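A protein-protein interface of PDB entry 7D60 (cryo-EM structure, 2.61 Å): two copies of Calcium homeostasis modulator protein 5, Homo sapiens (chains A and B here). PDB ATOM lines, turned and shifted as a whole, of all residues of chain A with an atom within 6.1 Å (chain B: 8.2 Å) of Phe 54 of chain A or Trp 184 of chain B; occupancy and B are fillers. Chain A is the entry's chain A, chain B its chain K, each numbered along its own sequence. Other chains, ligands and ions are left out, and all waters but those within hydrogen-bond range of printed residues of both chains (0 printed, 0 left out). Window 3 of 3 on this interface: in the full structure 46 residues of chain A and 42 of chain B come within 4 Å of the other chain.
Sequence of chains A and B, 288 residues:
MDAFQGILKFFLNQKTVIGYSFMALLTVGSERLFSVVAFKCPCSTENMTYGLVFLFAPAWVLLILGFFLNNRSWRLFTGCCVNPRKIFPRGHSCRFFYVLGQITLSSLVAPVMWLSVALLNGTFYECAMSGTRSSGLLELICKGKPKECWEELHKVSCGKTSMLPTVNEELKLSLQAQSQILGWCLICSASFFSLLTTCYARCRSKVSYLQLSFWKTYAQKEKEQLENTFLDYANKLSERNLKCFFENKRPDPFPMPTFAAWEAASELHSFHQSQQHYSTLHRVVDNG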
ATOM      1  N   PHE A  34       7.786 -14.495 -19.062  1.00  0.00           N
ATOM      2  CA  PHE A  34       8.443 -14.887 -20.301  1.00  0.00           C
ATOM      3  C   PHE A  34       7.506 -15.634 -21.233  1.00  0.00           C
ATOM      4  O   PHE A  34       7.597 -15.471 -22.452  1.00  0.00           O
ATOM      5  CB  PHE A  34       9.663 -15.756 -20.003  1.00  0.00           C
ATOM      6  CG  PHE A  34      10.936 -14.984 -19.883  1.00  0.00           C
ATOM      7  CD1 PHE A  34      11.573 -14.498 -21.009  1.00  0.00           C
ATOM      8  CD2 PHE A  34      11.498 -14.743 -18.643  1.00  0.00           C
ATOM      9  CE1 PHE A  34      12.747 -13.781 -20.900  1.00  0.00           C
ATOM     10  CE2 PHE A  34      12.671 -14.030 -18.526  1.00  0.00           C
ATOM     11  CZ  PHE A  34      13.296 -13.549 -19.656  1.00  0.00           C
ATOM     12  N   ALA A  38       6.783 -12.619 -24.010  1.00  0.00           N
ATOM     13  CA  ALA A  38       7.876 -12.743 -24.968  1.00  0.00           C
ATOM     14  C   ALA A  38       7.810 -14.001 -25.822  1.00  0.00           C
ATOM     15  O   ALA A  38       8.203 -13.964 -26.987  1.00  0.00           O
ATOM     16  CB  ALA A  38       9.219 -12.705 -24.239  1.00  0.00           C
ATOM     17  N   PHE A  39       7.342 -15.116 -25.278  1.00  0.00           N
ATOM     18  CA  PHE A  39       7.369 -16.379 -26.003  1.00  0.00           C
ATOM     19  C   PHE A  39       6.209 -16.438 -26.985  1.00  0.00           C
ATOM     20  O   PHE A  39       5.049 -16.268 -26.599  1.00  0.00           O
ATOM     21  CB  PHE A  39       7.307 -17.554 -25.032  1.00  0.00           C
ATOM     22  CG  PHE A  39       7.617 -18.884 -25.656  1.00  0.00           C
ATOM     23  CD1 PHE A  39       6.603 -19.719 -26.085  1.00  0.00           C
ATOM     24  CD2 PHE A  39       8.922 -19.308 -25.794  1.00  0.00           C
ATOM     25  CE1 PHE A  39       6.887 -20.940 -26.650  1.00  0.00           C
ATOM     26  CE2 PHE A  39       9.208 -20.535 -26.349  1.00  0.00           C
ATOM     27  CZ  PHE A  39       8.191 -21.346 -26.782  1.00  0.00           C
ATOM     28  N   THR A  49      15.174 -25.718 -31.722  1.00  0.00           N
ATOM     29  CA  THR A  49      16.158 -24.820 -31.127  1.00  0.00           C
ATOM     30  C   THR A  49      15.500 -23.692 -30.343  1.00  0.00           C
ATOM     31  O   THR A  49      16.048 -23.245 -29.336  1.00  0.00           O
ATOM     32  CB  THR A  49      17.062 -24.254 -32.218  1.00  0.00           C
ATOM     33  OG1 THR A  49      17.445 -25.309 -33.104  1.00  0.00           O
ATOM     34  CG2 THR A  49      18.312 -23.643 -31.628  1.00  0.00           C
ATOM     35  N   TYR A  50      14.327 -23.238 -30.768  1.00  0.00           N
ATOM     36  CA  TYR A  50      13.704 -22.087 -30.126  1.00  0.00           C
ATOM     37  C   TYR A  50      13.146 -22.428 -28.751  1.00  0.00           C
ATOM     38  O   TYR A  50      13.278 -21.635 -27.815  1.00  0.00           O
ATOM     39  CB  TYR A  50      12.603 -21.533 -31.021  1.00  0.00           C
ATOM     40  CG  TYR A  50      11.900 -20.326 -30.471  1.00  0.00           C
ATOM     41  CD1 TYR A  50      10.616 -20.420 -29.980  1.00  0.00           C
ATOM     42  CD2 TYR A  50      12.516 -19.091 -30.453  1.00  0.00           C
ATOM     43  CE1 TYR A  50       9.966 -19.320 -29.493  1.00  0.00           C
ATOM     44  CE2 TYR A  50      11.872 -17.986 -29.958  1.00  0.00           C
ATOM     45  CZ  TYR A  50      10.599 -18.109 -29.477  1.00  0.00           C
ATOM     46  OH  TYR A  50       9.948 -17.013 -28.981  1.00  0.00           O
ATOM     47  N   GLY A  51      12.515 -23.591 -28.604  1.00  0.00           N
ATOM     48  CA  GLY A  51      11.934 -23.939 -27.323  1.00  0.00           C
ATOM     49  C   GLY A  51      12.923 -24.487 -26.328  1.00  0.00           C
ATOM     50  O   GLY A  51      12.686 -24.401 -25.122  1.00  0.00           O
ATOM     51  N   LEU A  52      14.029 -25.034 -26.808  1.00  0.00           N
ATOM     52  CA  LEU A  52      15.057 -25.623 -25.972  1.00  0.00           C
ATOM     53  C   LEU A  52      16.073 -24.594 -25.495  1.00  0.00           C
ATOM     54  O   LEU A  52      16.902 -24.913 -24.643  1.00  0.00           O
ATOM     55  CB  LEU A  52      15.743 -26.736 -26.762  1.00  0.00           C
ATOM     56  CG  LEU A  52      16.538 -27.876 -26.171  1.00  0.00           C
ATOM     57  CD1 LEU A  52      15.603 -28.685 -25.335  1.00  0.00           C
ATOM     58  CD2 LEU A  52      17.060 -28.723 -27.297  1.00  0.00           C
ATOM     59  N   VAL A  53      16.030 -23.379 -26.032  1.00  0.00           N
ATOM     60  CA  VAL A  53      16.840 -22.265 -25.548  1.00  0.00           C
ATOM     61  C   VAL A  53      16.119 -21.504 -24.444  1.00  0.00           C
ATOM     62  O   VAL A  53      16.728 -21.124 -23.446  1.00  0.00           O
ATOM     63  CB  VAL A  53      17.223 -21.357 -26.742  1.00  0.00           C
ATOM     64  CG1 VAL A  53      17.557 -19.950 -26.314  1.00  0.00           C
ATOM     65  CG2 VAL A  53      18.411 -21.934 -27.467  1.00  0.00           C
ATOM     66  N   PHE A  54      14.803 -21.335 -24.547  1.00  0.00           N
ATOM     67  CA  PHE A  54      14.034 -20.713 -23.475  1.00  0.00           C
ATOM     68  C   PHE A  54      13.940 -21.582 -22.227  1.00  0.00           C
ATOM     69  O   PHE A  54      13.522 -21.086 -21.179  1.00  0.00           O
ATOM     70  CB  PHE A  54      12.626 -20.388 -23.958  1.00  0.00           C
ATOM     71  CG  PHE A  54      12.466 -18.999 -24.488  1.00  0.00           C
ATOM     72  CD1 PHE A  54      12.866 -18.683 -25.773  1.00  0.00           C
ATOM     73  CD2 PHE A  54      11.887 -18.016 -23.709  1.00  0.00           C
ATOM     74  CE1 PHE A  54      12.704 -17.414 -26.262  1.00  0.00           C
ATOM     75  CE2 PHE A  54      11.723 -16.747 -24.194  1.00  0.00           C
ATOM     76  CZ  PHE A  54      12.132 -16.445 -25.472  1.00  0.00           C
ATOM     77  N   LEU A  55      14.304 -22.856 -22.316  1.00  0.00           N
ATOM     78  CA  LEU A  55      14.322 -23.780 -21.194  1.00  0.00           C
ATOM     79  C   LEU A  55      15.660 -23.763 -20.464  1.00  0.00           C
ATOM     80  O   LEU A  55      15.698 -23.670 -19.235  1.00  0.00           O
ATOM     81  CB  LEU A  55      14.015 -25.190 -21.703  1.00  0.00           C
ATOM     82  CG  LEU A  55      13.293 -26.233 -20.858  1.00  0.00           C
ATOM     83  CD1 LEU A  55      12.048 -25.667 -20.236  1.00  0.00           C
ATOM     84  CD2 LEU A  55      12.951 -27.406 -21.737  1.00  0.00           C
ATOM     85  N   PHE A  56      16.765 -23.828 -21.203  1.00  0.00           N
ATOM     86  CA  PHE A  56      18.077 -24.061 -20.620  1.00  0.00           C
ATOM     87  C   PHE A  56      18.954 -22.821 -20.509  1.00  0.00           C
ATOM     88  O   PHE A  56      19.904 -22.834 -19.726  1.00  0.00           O
ATOM     89  CB  PHE A  56      18.828 -25.119 -21.429  1.00  0.00           C
ATOM     90  CG  PHE A  56      18.292 -26.500 -21.245  1.00  0.00           C
ATOM     91  CD1 PHE A  56      18.263 -27.079 -19.993  1.00  0.00           C
ATOM     92  CD2 PHE A  56      17.818 -27.222 -22.322  1.00  0.00           C
ATOM     93  CE1 PHE A  56      17.769 -28.353 -19.818  1.00  0.00           C
ATOM     94  CE2 PHE A  56      17.322 -28.496 -22.150  1.00  0.00           C
ATOM     95  CZ  PHE A  56      17.298 -29.059 -20.898  1.00  0.00           C
ATOM     96  N   ALA A  57      18.692 -21.772 -21.268  1.00  0.00           N
ATOM     97  CA  ALA A  57      19.527 -20.583 -21.146  1.00  0.00           C
ATOM     98  C   ALA A  57      19.232 -19.736 -19.904  1.00  0.00           C
ATOM     99  O   ALA A  57      20.181 -19.178 -19.348  1.00  0.00           O
ATOM    100  CB  ALA A  57      19.452 -19.720 -22.408  1.00  0.00           C
ATOM    101  N   PRO A  58      17.987 -19.574 -19.420  1.00  0.00           N
ATOM    102  CA  PRO A  58      17.839 -18.969 -18.088  1.00  0.00           C
ATOM    103  C   PRO A  58      18.292 -19.863 -16.947  1.00  0.00           C
ATOM    104  O   PRO A  58      18.443 -19.366 -15.829  1.00  0.00           O
ATOM    105  CB  PRO A  58      16.340 -18.674 -17.998  1.00  0.00           C
ATOM    106  CG  PRO A  58      15.932 -18.513 -19.360  1.00  0.00           C
ATOM    107  CD  PRO A  58      16.683 -19.543 -20.110  1.00  0.00           C
ATOM    108  N   VAL A  61      22.186 -19.009 -16.754  1.00  0.00           N
ATOM    109  CA  VAL A  61      22.459 -17.691 -16.196  1.00  0.00           C
ATOM    110  C   VAL A  61      22.288 -17.708 -14.682  1.00  0.00           C
ATOM    111  O   VAL A  61      23.066 -17.086 -13.949  1.00  0.00           O
ATOM    112  CB  VAL A  61      21.552 -16.653 -16.886  1.00  0.00           C
ATOM    113  CG1 VAL A  61      21.541 -15.324 -16.165  1.00  0.00           C
ATOM    114  CG2 VAL A  61      21.992 -16.462 -18.313  1.00  0.00           C
ATOM    115  N   TRP A 114      14.011 -23.414 -11.757  1.00  0.00           N
ATOM    116  CA  TRP A 114      13.550 -22.842 -13.016  1.00  0.00           C
ATOM    117  C   TRP A 114      13.013 -23.923 -13.939  1.00  0.00           C
ATOM    118  O   TRP A 114      11.963 -23.747 -14.560  1.00  0.00           O
ATOM    119  CB  TRP A 114      14.679 -22.073 -13.702  1.00  0.00           C
ATOM    120  CG  TRP A 114      14.410 -21.795 -15.148  1.00  0.00           C
ATOM    121  CD1 TRP A 114      14.896 -22.477 -16.221  1.00  0.00           C
ATOM    122  CD2 TRP A 114      13.577 -20.765 -15.675  1.00  0.00           C
ATOM    123  NE1 TRP A 114      14.415 -21.940 -17.379  1.00  0.00           N
ATOM    124  CE2 TRP A 114      13.602 -20.885 -17.071  1.00  0.00           C
ATOM    125  CE3 TRP A 114      12.812 -19.751 -15.099  1.00  0.00           C
ATOM    126  CZ2 TRP A 114      12.898 -20.030 -17.900  1.00  0.00           C
ATOM    127  CZ3 TRP A 114      12.115 -18.905 -15.922  1.00  0.00           C
ATOM    128  CH2 TRP A 114      12.161 -19.047 -17.309  1.00  0.00           C
ATOM    129  N   ALA A 118       9.081 -24.208 -15.387  1.00  0.00           N
ATOM    130  CA  ALA A 118       8.952 -24.113 -16.834  1.00  0.00           C
ATOM    131  C   ALA A 118       8.353 -25.376 -17.436  1.00  0.00           C
ATOM    132  O   ALA A 118       7.725 -25.311 -18.495  1.00  0.00           O
ATOM    133  CB  ALA A 118      10.310 -23.822 -17.464  1.00  0.00           C
ATOM    134  N   PHE A 124       6.981 -24.376 -23.247  1.00  0.00           N
ATOM    135  CA  PHE A 124       8.295 -24.518 -23.860  1.00  0.00           C
ATOM    136  C   PHE A 124       8.526 -25.927 -24.379  1.00  0.00           C
ATOM    137  O   PHE A 124       9.249 -26.108 -25.361  1.00  0.00           O
ATOM    138  CB  PHE A 124       9.411 -24.159 -22.874  1.00  0.00           C
ATOM    139  CG  PHE A 124       9.323 -22.768 -22.306  1.00  0.00           C
ATOM    140  CD1 PHE A 124       9.801 -22.509 -21.038  1.00  0.00           C
ATOM    141  CD2 PHE A 124       8.787 -21.726 -23.030  1.00  0.00           C
ATOM    142  CE1 PHE A 124       9.731 -21.245 -20.500  1.00  0.00           C
ATOM    143  CE2 PHE A 124       8.711 -20.460 -22.489  1.00  0.00           C
ATOM    144  CZ  PHE A 124       9.186 -20.222 -21.225  1.00  0.00           C
ATOM    145  N   LEU B 115      21.962  -4.260 -25.810  1.00  0.00           N
ATOM    146  CA  LEU B 115      21.896  -5.119 -26.982  1.00  0.00           C
ATOM    147  C   LEU B 115      21.124  -6.404 -26.734  1.00  0.00           C
ATOM    148  O   LEU B 115      20.654  -7.020 -27.689  1.00  0.00           O
ATOM    149  CB  LEU B 115      23.302  -5.465 -27.443  1.00  0.00           C
ATOM    150  CG  LEU B 115      23.925  -4.557 -28.486  1.00  0.00           C
ATOM    151  CD1 LEU B 115      25.413  -4.785 -28.535  1.00  0.00           C
ATOM    152  CD2 LEU B 115      23.304  -4.845 -29.829  1.00  0.00           C
ATOM    153  N   SER B 116      20.987  -6.824 -25.483  1.00  0.00           N
ATOM    154  CA  SER B 116      20.266  -8.041 -25.157  1.00  0.00           C
ATOM    155  C   SER B 116      18.771  -7.810 -25.032  1.00  0.00           C
ATOM    156  O   SER B 116      17.983  -8.637 -25.489  1.00  0.00           O
ATOM    157  CB  SER B 116      20.808  -8.626 -23.859  1.00  0.00           C
ATOM    158  OG  SER B 116      22.159  -9.003 -24.012  1.00  0.00           O
ATOM    159  N   LEU B 119      17.423  -7.209 -28.530  1.00  0.00           N
ATOM    160  CA  LEU B 119      17.314  -8.415 -29.336  1.00  0.00           C
ATOM    161  C   LEU B 119      16.264  -9.388 -28.818  1.00  0.00           C
ATOM    162  O   LEU B 119      15.791 -10.226 -29.587  1.00  0.00           O
ATOM    163  CB  LEU B 119      18.662  -9.127 -29.413  1.00  0.00           C
ATOM    164  CG  LEU B 119      19.671  -8.616 -30.433  1.00  0.00           C
ATOM    165  CD1 LEU B 119      20.992  -9.302 -30.230  1.00  0.00           C
ATOM    166  CD2 LEU B 119      19.189  -8.831 -31.839  1.00  0.00           C
ATOM    167  N   LEU B 120      15.889  -9.305 -27.544  1.00  0.00           N
ATOM    168  CA  LEU B 120      14.802 -10.118 -27.021  1.00  0.00           C
ATOM    169  C   LEU B 120      13.434  -9.535 -27.334  1.00  0.00           C
ATOM    170  O   LEU B 120      12.427 -10.220 -27.144  1.00  0.00           O
ATOM    171  CB  LEU B 120      14.936 -10.287 -25.507  1.00  0.00           C
ATOM    172  CG  LEU B 120      15.987 -11.248 -24.956  1.00  0.00           C
ATOM    173  CD1 LEU B 120      15.792 -11.421 -23.469  1.00  0.00           C
ATOM    174  CD2 LEU B 120      15.937 -12.580 -25.653  1.00  0.00           C
ATOM    175  N   GLN B 176      11.310 -12.892 -35.964  1.00  0.00           N
ATOM    176  CA  GLN B 176      11.193 -12.528 -34.562  1.00  0.00           C
ATOM    177  C   GLN B 176      11.736 -13.610 -33.641  1.00  0.00           C
ATOM    178  O   GLN B 176      12.020 -13.330 -32.475  1.00  0.00           O
ATOM    179  CB  GLN B 176       9.726 -12.237 -34.248  1.00  0.00           C
ATOM    180  CG  GLN B 176       9.441 -11.405 -33.018  1.00  0.00           C
ATOM    181  CD  GLN B 176       8.897 -12.230 -31.872  1.00  0.00           C
ATOM    182  OE1 GLN B 176       8.443 -13.357 -32.064  1.00  0.00           O
ATOM    183  NE2 GLN B 176       8.914 -11.662 -30.674  1.00  0.00           N
ATOM    184  N   ALA B 177      11.895 -14.834 -34.139  1.00  0.00           N
ATOM    185  CA  ALA B 177      12.472 -15.922 -33.371  1.00  0.00           C
ATOM    186  C   ALA B 177      13.961 -16.100 -33.612  1.00  0.00           C
ATOM    187  O   ALA B 177      14.640 -16.680 -32.766  1.00  0.00           O
ATOM    188  CB  ALA B 177      11.757 -17.238 -33.692  1.00  0.00           C
ATOM    189  N   GLN B 178      14.478 -15.631 -34.743  1.00  0.00           N
ATOM    190  CA  GLN B 178      15.917 -15.643 -34.961  1.00  0.00           C
ATOM    191  C   GLN B 178      16.627 -14.602 -34.112  1.00  0.00           C
ATOM    192  O   GLN B 178      17.801 -14.776 -33.783  1.00  0.00           O
ATOM    193  CB  GLN B 178      16.229 -15.392 -36.431  1.00  0.00           C
ATOM    194  CG  GLN B 178      16.440 -16.631 -37.251  1.00  0.00           C
ATOM    195  CD  GLN B 178      16.566 -16.320 -38.724  1.00  0.00           C
ATOM    196  OE1 GLN B 178      16.618 -15.159 -39.118  1.00  0.00           O
ATOM    197  NE2 GLN B 178      16.616 -17.356 -39.546  1.00  0.00           N
ATOM    198  N   SER B 179      15.941 -13.517 -33.761  1.00  0.00           N
ATOM    199  CA  SER B 179      16.548 -12.480 -32.944  1.00  0.00           C
ATOM    200  C   SER B 179      16.553 -12.855 -31.473  1.00  0.00           C
ATOM    201  O   SER B 179      17.468 -12.474 -30.740  1.00  0.00           O
ATOM    202  CB  SER B 179      15.811 -11.164 -33.132  1.00  0.00           C
ATOM    203  OG  SER B 179      14.740 -11.051 -32.227  1.00  0.00           O
ATOM    204  N   GLN B 180      15.535 -13.584 -31.019  1.00  0.00           N
ATOM    205  CA  GLN B 180      15.476 -13.981 -29.623  1.00  0.00           C
ATOM    206  C   GLN B 180      16.450 -15.102 -29.301  1.00  0.00           C
ATOM    207  O   GLN B 180      16.796 -15.285 -28.134  1.00  0.00           O
ATOM    208  CB  GLN B 180      14.055 -14.387 -29.262  1.00  0.00           C
ATOM    209  CG  GLN B 180      13.119 -13.218 -29.193  1.00  0.00           C
ATOM    210  CD  GLN B 180      11.733 -13.610 -28.781  1.00  0.00           C
ATOM    211  OE1 GLN B 180      11.231 -14.652 -29.179  1.00  0.00           O
ATOM    212  NE2 GLN B 180      11.101 -12.779 -27.974  1.00  0.00           N
ATOM    213  N   ILE B 181      16.902 -15.851 -30.301  1.00  0.00           N
ATOM    214  CA  ILE B 181      17.947 -16.839 -30.075  1.00  0.00           C
ATOM    215  C   ILE B 181      19.299 -16.151 -29.943  1.00  0.00           C
ATOM    216  O   ILE B 181      20.116 -16.516 -29.090  1.00  0.00           O
ATOM    217  CB  ILE B 181      17.919 -17.890 -31.202  1.00  0.00           C
ATOM    218  CG1 ILE B 181      16.690 -18.780 -31.051  1.00  0.00           C
ATOM    219  CG2 ILE B 181      19.160 -18.749 -31.216  1.00  0.00           C
ATOM    220  CD1 ILE B 181      16.421 -19.640 -32.247  1.00  0.00           C
ATOM    221  N   LEU B 182      19.541 -15.115 -30.747  1.00  0.00           N
ATOM    222  CA  LEU B 182      20.752 -14.313 -30.610  1.00  0.00           C
ATOM    223  C   LEU B 182      20.760 -13.479 -29.339  1.00  0.00           C
ATOM    224  O   LEU B 182      21.835 -13.126 -28.857  1.00  0.00           O
ATOM    225  CB  LEU B 182      20.917 -13.388 -31.809  1.00  0.00           C
ATOM    226  CG  LEU B 182      21.252 -14.021 -33.152  1.00  0.00           C
ATOM    227  CD1 LEU B 182      21.140 -12.979 -34.240  1.00  0.00           C
ATOM    228  CD2 LEU B 182      22.639 -14.611 -33.119  1.00  0.00           C
ATOM    229  N   GLY B 183      19.592 -13.143 -28.799  1.00  0.00           N
ATOM    230  CA  GLY B 183      19.547 -12.421 -27.545  1.00  0.00           C
ATOM    231  C   GLY B 183      19.929 -13.275 -26.358  1.00  0.00           C
ATOM    232  O   GLY B 183      20.420 -12.756 -25.356  1.00  0.00           O
ATOM    233  N   TRP B 184      19.709 -14.587 -26.445  1.00  0.00           N
ATOM    234  CA  TRP B 184      20.126 -15.492 -25.384  1.00  0.00           C
ATOM    235  C   TRP B 184      21.555 -15.973 -25.558  1.00  0.00           C
ATOM    236  O   TRP B 184      22.184 -16.353 -24.572  1.00  0.00           O
ATOM    237  CB  TRP B 184      19.193 -16.701 -25.302  1.00  0.00           C
ATOM    238  CG  TRP B 184      17.875 -16.421 -24.666  1.00  0.00           C
ATOM    239  CD1 TRP B 184      16.658 -16.494 -25.260  1.00  0.00           C
ATOM    240  CD2 TRP B 184      17.633 -16.029 -23.310  1.00  0.00           C
ATOM    241  NE1 TRP B 184      15.673 -16.166 -24.370  1.00  0.00           N
ATOM    242  CE2 TRP B 184      16.246 -15.879 -23.163  1.00  0.00           C
ATOM    243  CE3 TRP B 184      18.455 -15.793 -22.206  1.00  0.00           C
ATOM    244  CZ2 TRP B 184      15.662 -15.498 -21.963  1.00  0.00           C
ATOM    245  CZ3 TRP B 184      17.875 -15.416 -21.020  1.00  0.00           C
ATOM    246  CH2 TRP B 184      16.493 -15.271 -20.905  1.00  0.00           C
ATOM    247  N   CYS B 185      22.081 -15.970 -26.780  1.00  0.00           N
ATOM    248  CA  CYS B 185      23.478 -16.324 -26.986  1.00  0.00           C
ATOM    249  C   CYS B 185      24.417 -15.215 -26.549  1.00  0.00           C
ATOM    250  O   CYS B 185      25.604 -15.471 -26.341  1.00  0.00           O
ATOM    251  CB  CYS B 185      23.735 -16.655 -28.453  1.00  0.00           C
ATOM    252  SG  CYS B 185      23.308 -18.339 -28.931  1.00  0.00           S
ATOM    253  N   LEU B 186      23.918 -13.992 -26.420  1.00  0.00           N
ATOM    254  CA  LEU B 186      24.710 -12.875 -25.936  1.00  0.00           C
ATOM    255  C   LEU B 186      24.680 -12.777 -24.417  1.00  0.00           C
ATOM    256  O   LEU B 186      25.690 -12.428 -23.808  1.00  0.00           O
ATOM    257  CB  LEU B 186      24.210 -11.573 -26.563  1.00  0.00           C
ATOM    258  CG  LEU B 186      24.977 -10.290 -26.258  1.00  0.00           C
ATOM    259  CD1 LEU B 186      26.321 -10.298 -26.946  1.00  0.00           C
ATOM    260  CD2 LEU B 186      24.167  -9.093 -26.684  1.00  0.00           C
ATOM    261  N   ILE B 187      23.541 -13.084 -23.796  1.00  0.00           N
ATOM    262  CA  ILE B 187      23.462 -13.102 -22.339  1.00  0.00           C
ATOM    263  C   ILE B 187      24.283 -14.254 -21.773  1.00  0.00           C
ATOM    264  O   ILE B 187      24.964 -14.106 -20.753  1.00  0.00           O
ATOM    265  CB  ILE B 187      21.988 -13.176 -21.896  1.00  0.00           C
ATOM    266  CG1 ILE B 187      21.253 -11.910 -22.297  1.00  0.00           C
ATOM    267  CG2 ILE B 187      21.856 -13.325 -20.403  1.00  0.00           C
ATOM    268  CD1 ILE B 187      19.757 -12.003 -22.142  1.00  0.00           C
ATOM    269  N   CYS B 188      24.275 -15.401 -22.448  1.00  0.00           N
ATOM    270  CA  CYS B 188      24.966 -16.573 -21.930  1.00  0.00           C
ATOM    271  C   CYS B 188      26.476 -16.478 -22.084  1.00  0.00           C
ATOM    272  O   CYS B 188      27.209 -16.966 -21.220  1.00  0.00           O
ATOM    273  CB  CYS B 188      24.456 -17.834 -22.621  1.00  0.00           C
ATOM    274  SG  CYS B 188      22.857 -18.384 -22.032  1.00  0.00           S
ATOM    275  N   SER B 189      26.963 -15.868 -23.158  1.00  0.00           N
ATOM    276  CA  SER B 189      28.398 -15.782 -23.369  1.00  0.00           C
ATOM    277  C   SER B 189      29.030 -14.573 -22.696  1.00  0.00           C
ATOM    278  O   SER B 189      30.245 -14.571 -22.484  1.00  0.00           O
ATOM    279  CB  SER B 189      28.711 -15.759 -24.865  1.00  0.00           C
ATOM    280  OG  SER B 189      28.520 -14.470 -25.406  1.00  0.00           O
ATOM    281  N   ALA B 190      28.247 -13.551 -22.355  1.00  0.00           N
ATOM    282  CA  ALA B 190      28.795 -12.431 -21.601  1.00  0.00           C
ATOM    283  C   ALA B 190      28.769 -12.689 -20.103  1.00  0.00           C
ATOM    284  O   ALA B 190      29.562 -12.097 -19.370  1.00  0.00           O
ATOM    285  CB  ALA B 190      28.035 -11.144 -21.916  1.00  0.00           C
ATOM    286  N   SER B 191      27.866 -13.549 -19.630  1.00  0.00           N
ATOM    287  CA  SER B 191      27.898 -13.952 -18.229  1.00  0.00           C
ATOM    288  C   SER B 191      29.064 -14.884 -17.945  1.00  0.00           C
ATOM    289  O   SER B 191      29.643 -14.835 -16.857  1.00  0.00           O
ATOM    290  CB  SER B 191      26.586 -14.629 -17.842  1.00  0.00           C
ATOM    291  OG  SER B 191      25.528 -13.695 -17.789  1.00  0.00           O
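OE1 of Gln 180 of chain B lies within hydrogen-bond range of OH of Tyr 50 of chain A (2.7 Å). O of Ala 38 of chain A sits at hydrogen-bond distance from NE2 of Gln 180 of chain B, at 3.3 Å.
O of Trp 184 of chain B is in hydrogen-bond range of SG of Cys 188 of chain B (3.3 Å). The side-chain hydroxyl (OG) of Ser 191 of chain B sits at hydrogen-bond distance from the backbone carbonyl oxygen (O) of Ile 187 of chain B (3.0 Å). The backbone carbonyl oxygen of Leu 120 of chain B sits at hydrogen-bond distance from the side-chain amide nitrogen of Gln 180 of chain B (3.0 Å). The backbone NH of Phe 39 of chain A lies within hydrogen-bond range of the backbone carbonyl oxygen of Phe 34 of chain A (2.9 Å).
Among the printed residues, merely in contact across the chains: Phe 34 of chain A with Trp 184 of chain B, Pro 58 of chain A with Trp 184 of chain B, Ala 57 of chain A with Cys 188 of chain B, Phe 54 of chain A with Trp 184 of chain B, Val 53 of chain A with Trp 184 of chain B, Val 61 of chain A with Ile 187 of chain B and Tyr 50 of chain A with Ala 177 of chain B.
Phe 54 of chain A touches one residue of chain B. Of chain A, only Phe 34, Val 53, Phe 54 and Pro 58 come within 4 Å of Trp 184 of chain B. Printed residues of chain A within 4 Å of Ala 177 of chain B: Tyr 50 (3.8 Å). Of the printed residues of chain B, Phe 34 of chain A touches Trp 184. Of the printed residues of chain A, Cys 188 of chain B touches Ala 57 (3.7 Å). Of the printed residues of chain A, Ile 187 of chain B touches Val 61. Of the printed residues of chain B, Ala 38 of chain A touches Gln 180. The nearest residue of chain B that does not touch Phe 54 of chain A is Gln 180 of chain B (4.2 Å). The nearest residue of chain A that does not touch Trp 184 of chain B is Ala 57 of chain A (4.1 Å). The nearest printed residue of chain B that does not touch Tyr 50 of chain A is Ile 181 of chain B (4.2 Å).
Hydrophobic or aromatic side chains of chain B that line the printed part of chain A: Ala 177, Trp 184 and Ile 187. Of the 17 printed residues of chain A, 8 touch a printed residue of chain B. Among the printed residues, 9 pairs touch across the chains. Among the printed residues, no Asp or Glu carboxylate lies within 4 Å of a Lys or Arg side-chain nitrogen of the other chain.
No position is printed for both chains.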
